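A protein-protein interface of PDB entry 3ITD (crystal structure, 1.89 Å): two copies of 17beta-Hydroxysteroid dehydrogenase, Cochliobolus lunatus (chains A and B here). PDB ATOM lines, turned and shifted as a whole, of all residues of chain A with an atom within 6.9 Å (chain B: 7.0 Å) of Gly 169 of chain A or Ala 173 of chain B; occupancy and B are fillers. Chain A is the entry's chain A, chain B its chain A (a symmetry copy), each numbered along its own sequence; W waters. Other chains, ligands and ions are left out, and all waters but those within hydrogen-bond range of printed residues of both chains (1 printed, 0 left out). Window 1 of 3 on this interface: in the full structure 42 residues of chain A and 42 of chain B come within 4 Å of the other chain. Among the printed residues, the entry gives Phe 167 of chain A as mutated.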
ATOM      1  N   PHE A 124     -18.717 -17.869 -34.781  1.00  0.00           N
ATOM      2  CA  PHE A 124     -17.974 -18.177 -33.557  1.00  0.00           C
ATOM      3  C   PHE A 124     -16.477 -18.399 -33.817  1.00  0.00           C
ATOM      4  O   PHE A 124     -15.645 -18.096 -32.953  1.00  0.00           O
ATOM      5  CB  PHE A 124     -18.611 -19.371 -32.822  1.00  0.00           C
ATOM      6  CG  PHE A 124     -19.556 -18.943 -31.740  1.00  0.00           C
ATOM      7  CD1 PHE A 124     -20.787 -18.363 -32.067  1.00  0.00           C
ATOM      8  CD2 PHE A 124     -19.176 -19.031 -30.391  1.00  0.00           C
ATOM      9  CE1 PHE A 124     -21.657 -17.903 -31.072  1.00  0.00           C
ATOM     10  CE2 PHE A 124     -20.028 -18.586 -29.387  1.00  0.00           C
ATOM     11  CZ  PHE A 124     -21.282 -18.014 -29.719  1.00  0.00           C
ATOM     12  N   THR A 128     -15.209 -15.288 -31.454  1.00  0.00           N
ATOM     13  CA  THR A 128     -15.110 -15.834 -30.100  1.00  0.00           C
ATOM     14  C   THR A 128     -13.832 -16.686 -30.008  1.00  0.00           C
ATOM     15  O   THR A 128     -12.943 -16.375 -29.228  1.00  0.00           O
ATOM     16  CB  THR A 128     -16.380 -16.673 -29.760  1.00  0.00           C
ATOM     17  OG1 THR A 128     -17.556 -15.880 -30.013  1.00  0.00           O
ATOM     18  CG2 THR A 128     -16.378 -17.154 -28.288  1.00  0.00           C
ATOM     19  N   THR A 155     -24.526  -5.240 -28.083  1.00  0.00           N
ATOM     20  CA  THR A 155     -25.569  -6.258 -28.209  1.00  0.00           C
ATOM     21  C   THR A 155     -25.338  -7.423 -27.258  1.00  0.00           C
ATOM     22  O   THR A 155     -26.243  -8.230 -27.043  1.00  0.00           O
ATOM     23  CB  THR A 155     -25.711  -6.798 -29.662  1.00  0.00           C
ATOM     24  OG1 THR A 155     -24.476  -7.405 -30.037  1.00  0.00           O
ATOM     25  CG2 THR A 155     -26.057  -5.641 -30.622  1.00  0.00           C
ATOM     26  N   SER A 156     -24.140  -7.503 -26.670  1.00  0.00           N
ATOM     27  CA  SER A 156     -23.846  -8.586 -25.745  1.00  0.00           C
ATOM     28  C   SER A 156     -24.764  -8.553 -24.504  1.00  0.00           C
ATOM     29  O   SER A 156     -25.381  -9.577 -24.135  1.00  0.00           O
ATOM     30  CB  SER A 156     -22.358  -8.573 -25.378  1.00  0.00           C
ATOM     31  OG  SER A 156     -22.176  -9.221 -24.140  1.00  0.00           O
ATOM     32  N   HIS A 164     -30.856 -11.584 -33.692  1.00  0.00           N
ATOM     33  CA  HIS A 164     -29.458 -11.225 -33.570  1.00  0.00           C
ATOM     34  C   HIS A 164     -28.828 -12.083 -32.457  1.00  0.00           C
ATOM     35  O   HIS A 164     -27.829 -11.714 -31.842  1.00  0.00           O
ATOM     36  CB  HIS A 164     -29.370  -9.703 -33.301  1.00  0.00           C
ATOM     37  CG  HIS A 164     -28.041  -9.066 -33.624  1.00  0.00           C
ATOM     38  ND1 HIS A 164     -27.280  -9.403 -34.726  1.00  0.00           N
ATOM     39  CD2 HIS A 164     -27.376  -8.051 -33.007  1.00  0.00           C
ATOM     40  CE1 HIS A 164     -26.192  -8.646 -34.757  1.00  0.00           C
ATOM     41  NE2 HIS A 164     -26.227  -7.817 -33.726  1.00  0.00           N
ATOM     42  N   SER A 165     -29.391 -13.275 -32.228  1.00  0.00           N
ATOM     43  CA  SER A 165     -28.930 -14.093 -31.109  1.00  0.00           C
ATOM     44  C   SER A 165     -27.489 -14.610 -31.273  1.00  0.00           C
ATOM     45  O   SER A 165     -26.702 -14.601 -30.332  1.00  0.00           O
ATOM     46  CB  SER A 165     -29.909 -15.250 -30.843  1.00  0.00           C
ATOM     47  OG  SER A 165     -29.875 -16.209 -31.891  1.00  0.00           O
ATOM     48  N   LEU A 166     -27.160 -15.067 -32.476  1.00  0.00           N
ATOM     49  CA  LEU A 166     -25.866 -15.674 -32.746  1.00  0.00           C
ATOM     50  C   LEU A 166     -24.723 -14.690 -32.475  1.00  0.00           C
ATOM     51  O   LEU A 166     -23.764 -14.995 -31.764  1.00  0.00           O
ATOM     52  CB  LEU A 166     -25.838 -16.175 -34.206  1.00  0.00           C
ATOM     53  CG  LEU A 166     -24.521 -16.892 -34.552  1.00  0.00           C
ATOM     54  CD1 LEU A 166     -24.386 -18.157 -33.727  1.00  0.00           C
ATOM     55  CD2 LEU A 166     -24.600 -17.278 -36.010  1.00  0.00           C
ATOM     56  N   PHE A 167     -24.852 -13.480 -33.020  1.00  0.00           N
ATOM     57  CA  PHE A 167     -23.815 -12.482 -32.857  1.00  0.00           C
ATOM     58  C   PHE A 167     -23.762 -12.006 -31.389  1.00  0.00           C
ATOM     59  O   PHE A 167     -22.679 -11.892 -30.806  1.00  0.00           O
ATOM     60  CB  PHE A 167     -24.065 -11.300 -33.826  1.00  0.00           C
ATOM     61  CG  PHE A 167     -23.068 -10.173 -33.678  1.00  0.00           C
ATOM     62  CD1 PHE A 167     -21.870 -10.181 -34.401  1.00  0.00           C
ATOM     63  CD2 PHE A 167     -23.311  -9.123 -32.783  1.00  0.00           C
ATOM     64  CE1 PHE A 167     -20.929  -9.139 -34.257  1.00  0.00           C
ATOM     65  CE2 PHE A 167     -22.387  -8.064 -32.633  1.00  0.00           C
ATOM     66  CZ  PHE A 167     -21.187  -8.072 -33.370  1.00  0.00           C
ATOM     67  N   SER A 168     -24.921 -11.735 -30.802  1.00  0.00           N
ATOM     68  CA  SER A 168     -24.987 -11.318 -29.388  1.00  0.00           C
ATOM     69  C   SER A 168     -24.277 -12.296 -28.455  1.00  0.00           C
ATOM     70  O   SER A 168     -23.496 -11.874 -27.579  1.00  0.00           O
ATOM     71  CB  SER A 168     -26.442 -11.104 -28.945  1.00  0.00           C
ATOM     72  OG  SER A 168     -27.049 -10.096 -29.767  1.00  0.00           O
ATOM     73  N   GLY A 169     -24.537 -13.592 -28.655  1.00  0.00           N
ATOM     74  CA  GLY A 169     -23.868 -14.650 -27.871  1.00  0.00           C
ATOM     75  C   GLY A 169     -22.356 -14.721 -28.108  1.00  0.00           C
ATOM     76  O   GLY A 169     -21.570 -14.947 -27.186  1.00  0.00           O
ATOM     77  N   SER A 170     -21.940 -14.540 -29.358  1.00  0.00           N
ATOM     78  CA  SER A 170     -20.508 -14.569 -29.694  1.00  0.00           C
ATOM     79  C   SER A 170     -19.739 -13.494 -28.913  1.00  0.00           C
ATOM     80  O   SER A 170     -18.583 -13.726 -28.517  1.00  0.00           O
ATOM     81  CB  SER A 170     -20.273 -14.450 -31.225  1.00  0.00           C
ATOM     82  OG  SER A 170     -20.338 -13.070 -31.663  1.00  0.00           O
ATOM     83  N   LYS A 171     -20.393 -12.362 -28.632  1.00  0.00           N
ATOM     84  CA  LYS A 171     -19.769 -11.291 -27.821  1.00  0.00           C
ATOM     85  C   LYS A 171     -19.982 -11.455 -26.314  1.00  0.00           C
ATOM     86  O   LYS A 171     -19.145 -11.011 -25.545  1.00  0.00           O
ATOM     87  CB  LYS A 171     -20.226  -9.898 -28.307  1.00  0.00           C
ATOM     88  CG  LYS A 171     -19.832  -9.606 -29.803  1.00  0.00           C
ATOM     89  CD  LYS A 171     -18.389 -10.044 -30.132  1.00  0.00           C
ATOM     90  CE  LYS A 171     -18.046  -9.807 -31.617  1.00  0.00           C
ATOM     91  NZ  LYS A 171     -17.369  -8.537 -31.827  1.00  0.00           N
ATOM     92  N   GLY A 172     -21.085 -12.079 -25.891  1.00  0.00           N
ATOM     93  CA  GLY A 172     -21.275 -12.397 -24.453  1.00  0.00           C
ATOM     94  C   GLY A 172     -20.132 -13.265 -23.948  1.00  0.00           C
ATOM     95  O   GLY A 172     -19.633 -13.095 -22.829  1.00  0.00           O
ATOM     96  N   ALA A 173     -19.687 -14.200 -24.784  1.00  0.00           N
ATOM     97  CA  ALA A 173     -18.526 -15.010 -24.447  1.00  0.00           C
ATOM     98  C   ALA A 173     -17.281 -14.165 -24.162  1.00  0.00           C
ATOM     99  O   ALA A 173     -16.569 -14.412 -23.191  1.00  0.00           O
ATOM    100  CB  ALA A 173     -18.237 -16.060 -25.551  1.00  0.00           C
ATOM    101  N   VAL A 174     -17.002 -13.207 -25.039  1.00  0.00           N
ATOM    102  CA  VAL A 174     -15.834 -12.307 -24.908  1.00  0.00           C
ATOM    103  C   VAL A 174     -15.875 -11.517 -23.588  1.00  0.00           C
ATOM    104  O   VAL A 174     -14.824 -11.352 -22.941  1.00  0.00           O
ATOM    105  CB  VAL A 174     -15.719 -11.325 -26.135  1.00  0.00           C
ATOM    106  CG1 VAL A 174     -14.574 -10.317 -25.956  1.00  0.00           C
ATOM    107  CG2 VAL A 174     -15.505 -12.153 -27.413  1.00  0.00           C
ATOM    108  N   SER A 176     -17.133 -12.403 -20.740  1.00  0.00           N
ATOM    109  CA  SER A 176     -16.732 -13.332 -19.661  1.00  0.00           C
ATOM    110  C   SER A 176     -15.242 -13.648 -19.776  1.00  0.00           C
ATOM    111  O   SER A 176     -14.506 -13.585 -18.765  1.00  0.00           O
ATOM    112  CB  SER A 176     -17.589 -14.606 -19.723  1.00  0.00           C
ATOM    113  OG  SER A 176     -18.933 -14.323 -19.361  1.00  0.00           O
ATOM    114  N   PHE B 124     -16.753 -25.716 -26.182  1.00  0.00           N
ATOM    115  CA  PHE B 124     -17.743 -24.891 -26.878  1.00  0.00           C
ATOM    116  C   PHE B 124     -18.734 -25.728 -27.699  1.00  0.00           C
ATOM    117  O   PHE B 124     -19.898 -25.336 -27.855  1.00  0.00           O
ATOM    118  CB  PHE B 124     -17.048 -23.819 -27.737  1.00  0.00           C
ATOM    119  CG  PHE B 124     -16.938 -22.500 -27.034  1.00  0.00           C
ATOM    120  CD1 PHE B 124     -16.056 -22.345 -25.957  1.00  0.00           C
ATOM    121  CD2 PHE B 124     -17.783 -21.436 -27.387  1.00  0.00           C
ATOM    122  CE1 PHE B 124     -15.982 -21.139 -25.250  1.00  0.00           C
ATOM    123  CE2 PHE B 124     -17.721 -20.228 -26.701  1.00  0.00           C
ATOM    124  CZ  PHE B 124     -16.816 -20.067 -25.622  1.00  0.00           C
ATOM    125  N   ASN B 127     -21.256 -27.013 -24.679  1.00  0.00           N
ATOM    126  CA  ASN B 127     -21.791 -25.999 -23.749  1.00  0.00           C
ATOM    127  C   ASN B 127     -22.497 -24.842 -24.422  1.00  0.00           C
ATOM    128  O   ASN B 127     -23.400 -24.247 -23.841  1.00  0.00           O
ATOM    129  CB  ASN B 127     -20.653 -25.375 -22.920  1.00  0.00           C
ATOM    130  CG  ASN B 127     -20.050 -26.344 -21.907  1.00  0.00           C
ATOM    131  OD1 ASN B 127     -20.243 -27.534 -22.011  1.00  0.00           O
ATOM    132  ND2 ASN B 127     -19.251 -25.823 -20.963  1.00  0.00           N
ATOM    133  N   THR B 128     -22.071 -24.508 -25.638  1.00  0.00           N
ATOM    134  CA  THR B 128     -22.502 -23.266 -26.282  1.00  0.00           C
ATOM    135  C   THR B 128     -23.204 -23.619 -27.604  1.00  0.00           C
ATOM    136  O   THR B 128     -24.381 -23.328 -27.769  1.00  0.00           O
ATOM    137  CB  THR B 128     -21.280 -22.325 -26.517  1.00  0.00           C
ATOM    138  OG1 THR B 128     -20.565 -22.154 -25.279  1.00  0.00           O
ATOM    139  CG2 THR B 128     -21.712 -20.945 -27.071  1.00  0.00           C
ATOM    140  N   SER B 152     -26.553 -22.070 -17.703  1.00  0.00           N
ATOM    141  CA  SER B 152     -25.409 -21.188 -17.647  1.00  0.00           C
ATOM    142  C   SER B 152     -24.618 -21.588 -16.396  1.00  0.00           C
ATOM    143  O   SER B 152     -24.549 -22.785 -16.058  1.00  0.00           O
ATOM    144  CB  SER B 152     -25.897 -19.723 -17.629  1.00  0.00           C
ATOM    145  OG  SER B 152     -24.808 -18.832 -17.499  1.00  0.00           O
ATOM    146  N   SER B 156     -20.261 -17.382 -15.188  1.00  0.00           N
ATOM    147  CA  SER B 156     -20.438 -16.543 -16.363  1.00  0.00           C
ATOM    148  C   SER B 156     -20.251 -15.045 -16.039  1.00  0.00           C
ATOM    149  O   SER B 156     -19.487 -14.331 -16.726  1.00  0.00           O
ATOM    150  CB  SER B 156     -21.791 -16.841 -17.020  1.00  0.00           C
ATOM    151  OG  SER B 156     -22.195 -15.726 -17.782  1.00  0.00           O
ATOM    152  N   LYS B 157     -20.907 -14.581 -14.965  1.00  0.00           N
ATOM    153  CA  LYS B 157     -20.867 -13.161 -14.566  1.00  0.00           C
ATOM    154  C   LYS B 157     -20.592 -12.942 -13.084  1.00  0.00           C
ATOM    155  O   LYS B 157     -19.986 -11.942 -12.711  1.00  0.00           O
ATOM    156  CB  LYS B 157     -22.207 -12.469 -14.885  1.00  0.00           C
ATOM    157  CG  LYS B 157     -22.545 -12.487 -16.362  1.00  0.00           C
ATOM    158  CD  LYS B 157     -23.905 -11.840 -16.658  1.00  0.00           C
ATOM    159  CE  LYS B 157     -24.003 -11.562 -18.174  1.00  0.00           C
ATOM    160  NZ  LYS B 157     -23.340 -12.653 -19.037  1.00  0.00           N
ATOM    161  N   SER B 168     -16.083 -20.263 -18.323  1.00  0.00           N
ATOM    162  CA  SER B 168     -16.813 -19.013 -18.035  1.00  0.00           C
ATOM    163  C   SER B 168     -17.370 -18.356 -19.295  1.00  0.00           C
ATOM    164  O   SER B 168     -18.548 -17.946 -19.322  1.00  0.00           O
ATOM    165  CB  SER B 168     -15.930 -18.029 -17.253  1.00  0.00           C
ATOM    166  OG  SER B 168     -15.516 -18.633 -16.019  1.00  0.00           O
ATOM    167  N   GLY B 169     -16.531 -18.271 -20.333  1.00  0.00           N
ATOM    168  CA  GLY B 169     -16.958 -17.720 -21.635  1.00  0.00           C
ATOM    169  C   GLY B 169     -18.034 -18.561 -22.329  1.00  0.00           C
ATOM    170  O   GLY B 169     -18.964 -18.035 -22.945  1.00  0.00           O
ATOM    171  N   SER B 170     -17.906 -19.882 -22.244  1.00  0.00           N
ATOM    172  CA  SER B 170     -18.894 -20.783 -22.857  1.00  0.00           C
ATOM    173  C   SER B 170     -20.296 -20.532 -22.284  1.00  0.00           C
ATOM    174  O   SER B 170     -21.293 -20.634 -23.022  1.00  0.00           O
ATOM    175  CB  SER B 170     -18.475 -22.273 -22.727  1.00  0.00           C
ATOM    176  OG  SER B 170     -18.814 -22.804 -21.423  1.00  0.00           O
ATOM    177  N   LYS B 171     -20.370 -20.140 -21.008  1.00  0.00           N
ATOM    178  CA  LYS B 171     -21.668 -19.801 -20.379  1.00  0.00           C
ATOM    179  C   LYS B 171     -22.076 -18.337 -20.558  1.00  0.00           C
ATOM    180  O   LYS B 171     -23.262 -18.049 -20.580  1.00  0.00           O
ATOM    181  CB  LYS B 171     -21.679 -20.213 -18.890  1.00  0.00           C
ATOM    182  CG  LYS B 171     -21.475 -21.759 -18.675  1.00  0.00           C
ATOM    183  CD  LYS B 171     -22.302 -22.609 -19.663  1.00  0.00           C
ATOM    184  CE  LYS B 171     -22.037 -24.117 -19.476  1.00  0.00           C
ATOM    185  NZ  LYS B 171     -23.023 -24.742 -18.608  1.00  0.00           N
ATOM    186  N   GLY B 172     -21.113 -17.417 -20.679  1.00  0.00           N
ATOM    187  CA  GLY B 172     -21.446 -16.006 -21.000  1.00  0.00           C
ATOM    188  C   GLY B 172     -22.211 -15.929 -22.313  1.00  0.00           C
ATOM    189  O   GLY B 172     -23.162 -15.152 -22.465  1.00  0.00           O
ATOM    190  N   ALA B 173     -21.815 -16.756 -23.277  1.00  0.00           N
ATOM    191  CA  ALA B 173     -22.547 -16.844 -24.532  1.00  0.00           C
ATOM    192  C   ALA B 173     -24.020 -17.212 -24.330  1.00  0.00           C
ATOM    193  O   ALA B 173     -24.902 -16.609 -24.936  1.00  0.00           O
ATOM    194  CB  ALA B 173     -21.862 -17.833 -25.511  1.00  0.00           C
ATOM    195  N   VAL B 174     -24.269 -18.233 -23.517  1.00  0.00           N
ATOM    196  CA  VAL B 174     -25.637 -18.714 -23.220  1.00  0.00           C
ATOM    197  C   VAL B 174     -26.503 -17.604 -22.598  1.00  0.00           C
ATOM    198  O   VAL B 174     -27.691 -17.484 -22.954  1.00  0.00           O
ATOM    199  CB  VAL B 174     -25.615 -19.983 -22.287  1.00  0.00           C
ATOM    200  CG1 VAL B 174     -27.030 -20.425 -21.886  1.00  0.00           C
ATOM    201  CG2 VAL B 174     -24.888 -21.124 -23.019  1.00  0.00           C
ATOM    202  N   ASP B 175     -25.926 -16.817 -21.685  1.00  0.00           N
ATOM    203  CA  ASP B 175     -26.651 -15.682 -21.068  1.00  0.00           C
ATOM    204  C   ASP B 175     -27.209 -14.753 -22.127  1.00  0.00           C
ATOM    205  O   ASP B 175     -28.402 -14.351 -22.077  1.00  0.00           O
ATOM    206  CB  ASP B 175     -25.744 -14.854 -20.134  1.00  0.00           C
ATOM    207  CG  ASP B 175     -25.364 -15.585 -18.855  1.00  0.00           C
ATOM    208  OD1 ASP B 175     -25.816 -16.735 -18.645  1.00  0.00           O
ATOM    209  OD2 ASP B 175     -24.602 -14.991 -18.048  1.00  0.00           O
ATOM    210  N   SER B 176     -26.348 -14.408 -23.086  1.00  0.00           N
ATOM    211  CA  SER B 176     -26.742 -13.495 -24.181  1.00  0.00           C
ATOM    212  C   SER B 176     -27.750 -14.187 -25.096  1.00  0.00           C
ATOM    213  O   SER B 176     -28.799 -13.594 -25.438  1.00  0.00           O
ATOM    214  CB  SER B 176     -25.495 -13.037 -24.954  1.00  0.00           C
ATOM    215  OG  SER B 176     -24.695 -12.181 -24.151  1.00  0.00           O
ATOM    216  N   PHE B 177     -27.480 -15.452 -25.453  1.00  0.00           N
ATOM    217  CA  PHE B 177     -28.429 -16.220 -26.257  1.00  0.00           C
ATOM    218  C   PHE B 177     -29.856 -16.113 -25.702  1.00  0.00           C
ATOM    219  O   PHE B 177     -30.799 -15.810 -26.456  1.00  0.00           O
ATOM    220  CB  PHE B 177     -28.093 -17.725 -26.354  1.00  0.00           C
ATOM    221  CG  PHE B 177     -26.868 -18.088 -27.189  1.00  0.00           C
ATOM    222  CD1 PHE B 177     -26.404 -17.274 -28.236  1.00  0.00           C
ATOM    223  CD2 PHE B 177     -26.237 -19.302 -26.963  1.00  0.00           C
ATOM    224  CE1 PHE B 177     -25.299 -17.679 -29.008  1.00  0.00           C
ATOM    225  CE2 PHE B 177     -25.102 -19.712 -27.725  1.00  0.00           C
ATOM    226  CZ  PHE B 177     -24.637 -18.878 -28.738  1.00  0.00           C
ATOM    227  N   VAL B 178     -30.042 -16.401 -24.402  1.00  0.00           N
ATOM    228  CA  VAL B 178     -31.418 -16.542 -23.909  1.00  0.00           C
ATOM    229  C   VAL B 178     -32.197 -15.230 -23.980  1.00  0.00           C
ATOM    230  O   VAL B 178     -33.394 -15.241 -24.285  1.00  0.00           O
ATOM    231  CB  VAL B 178     -31.584 -17.253 -22.505  1.00  0.00           C
ATOM    232  CG1 VAL B 178     -30.966 -18.683 -22.529  1.00  0.00           C
ATOM    233  CG2 VAL B 178     -31.039 -16.444 -21.366  1.00  0.00           C
ATOM    234  N   ILE B 180     -31.948 -12.928 -26.227  1.00  0.00           N
ATOM    235  CA  ILE B 180     -32.393 -12.694 -27.612  1.00  0.00           C
ATOM    236  C   ILE B 180     -33.350 -13.802 -28.107  1.00  0.00           C
ATOM    237  O   ILE B 180     -34.297 -13.518 -28.852  1.00  0.00           O
ATOM    238  CB  ILE B 180     -31.201 -12.468 -28.588  1.00  0.00           C
ATOM    239  CG1 ILE B 180     -30.209 -11.431 -28.005  1.00  0.00           C
ATOM    240  CG2 ILE B 180     -31.690 -12.065 -29.996  1.00  0.00           C
ATOM    241  CD1 ILE B 180     -30.822 -10.111 -27.555  1.00  0.00           C
HETATM  242  O   HOH W   1     -20.652 -12.110 -19.527  1.00  0.00           O
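Printed residues of chain B that touch a printed residue of chain A: Phe 124, Thr 128, Ser 156, Ser 168, Gly 169, Gly 172, Ala 173, Ser 176, Phe 177 and Ile 180. Hydrophobic or aromatic side chains of chain B that line the printed part of chain A: Phe 124, Ala 173, Phe 177 and Ile 180.
Among the printed residues, merely in contact across the chains: Phe 124 of chain A with Phe 124 of chain B (3.9 Å), Phe 124 of chain A with Thr 128 of chain B (3.7 Å), Phe 124 of chain A with Phe 177 of chain B (3.6 Å), Thr 128 of chain A with Phe 124 of chain B (3.7 Å), His 164 of chain A with Ile 180 of chain B (3.8 Å), Ser 165 of chain A with Phe 177 of chain B (3.4 Å), Ser 165 of chain A with Ile 180 of chain B (3.4 Å), Ser 168 of chain A with Ser 176 of chain B (3.5 Å), Ser 168 of chain A with Ile 180 of chain B (3.9 Å), Gly 169 of chain A with Ala 173 of chain B (3.3 Å), Gly 169 of chain A with Ser 176 of chain B (3.7 Å), Gly 169 of chain A with Phe 177 of chain B (3.5 Å), Gly 172 of chain A with Gly 172 of chain B (3.8 Å), Gly 172 of chain A with Ala 173 of chain B (3.9 Å), Gly 172 of chain A with Ser 176 of chain B (3.4 Å), Ala 173 of chain A with Gly 169 of chain B (3.3 Å), Ala 173 of chain A with Gly 172 of chain B (3.9 Å), Ala 173 of chain A with Ala 173 of chain B (3.7 Å), Ser 176 of chain A with Ser 168 of chain B (3.5 Å), Ser 176 of chain A with Gly 169 of chain B (3.7 Å) and Ser 176 of chain A with Gly 172 of chain B (3.4 Å).
Of chain B, only Ala 173 (3.3 Å), Ser 176 (3.7 Å) and Phe 177 (3.5 Å) come within 4 Å of Gly 169 of chain A. Of the printed residues of chain B, Ala 173 of chain A touches Gly 169, Gly 172 and Ala 173. Of the printed residues of chain A, Thr 128 of chain B touches Phe 124. Ser 152 of chain B touches none of the printed residues of chain A. Printed residues of chain A within 4 Å of Ser 156 of chain B: Ser 176. Of the printed residues of chain A, Gly 169 of chain B touches Ala 173 (3.3 Å) and Ser 176 (3.7 Å). Lys 171 of chain B touches none of the printed residues of chain A. Gly 172 of chain B touches just these residues of chain A: Gly 172 (3.8 Å), Ala 173 (3.9 Å) and Ser 176 (3.4 Å). The nearest residue of chain B that does not touch Gly 169 of chain A is Gly 172 of chain B (5.0 Å). The nearest residue of chain A that does not touch Ala 173 of chain B is Phe 124 of chain A (4.3 Å). The nearest printed residue of chain A that does not touch Thr 128 of chain B is Gly 169 of chain A (6.0 Å).
The backbone carbonyl oxygen of Ser 156 of chain A is in hydrogen-bond range of the side-chain hydroxyl of Ser 176 of chain B. The backbone carbonyl oxygen (O) of Ser 156 of chain B is in hydrogen-bond range of the side-chain hydroxyl (OG) of Ser 176 of chain A, 2.7 Å away.
The side-chain hydroxyl (OG) of Ser 156 of chain B lies within hydrogen-bond range of the side-chain carboxylate (OD2) of Asp 175 of chain B (2.5 Å). O of Thr 155 of chain A lies within hydrogen-bond range of OG of Ser 168 of chain A. OG1 of Thr 128 of chain B lies within hydrogen-bond range of O of Ser 170 of chain B, at 2.8 Å. The backbone carbonyl oxygen (O) of His 164 of chain A lies within hydrogen-bond range of the side-chain hydroxyl (OG) of Ser 168 of chain A, at 2.7 Å. The side-chain hydroxyl (OG1) of Thr 128 of chain A lies within hydrogen-bond range of the backbone carbonyl oxygen (O) of Ser 170 of chain A (2.8 Å).
Water W1 lies within hydrogen-bond range of NZ of Lys 157 of chain B and OG of Ser 176 of chain A.
Phe 124 of chain B touches its own counterpart, Phe 124 of chain A. Ser 168 of chain A touches Ser 176 of chain B, and with the chains exchanged Ser 176 of chain A touches Ser 168 of chain B. Gly 169 of chain A touches Ser 176 of chain B, and with the chains exchanged Ser 176 of chain A touches Gly 169 of chain B. Gly 172 of chain A touches its own counterpart, Gly 172 of chain B. Of the 23 pairs that touch across the chains among the printed residues, 17 have their exchanged pair printed and touching as well.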
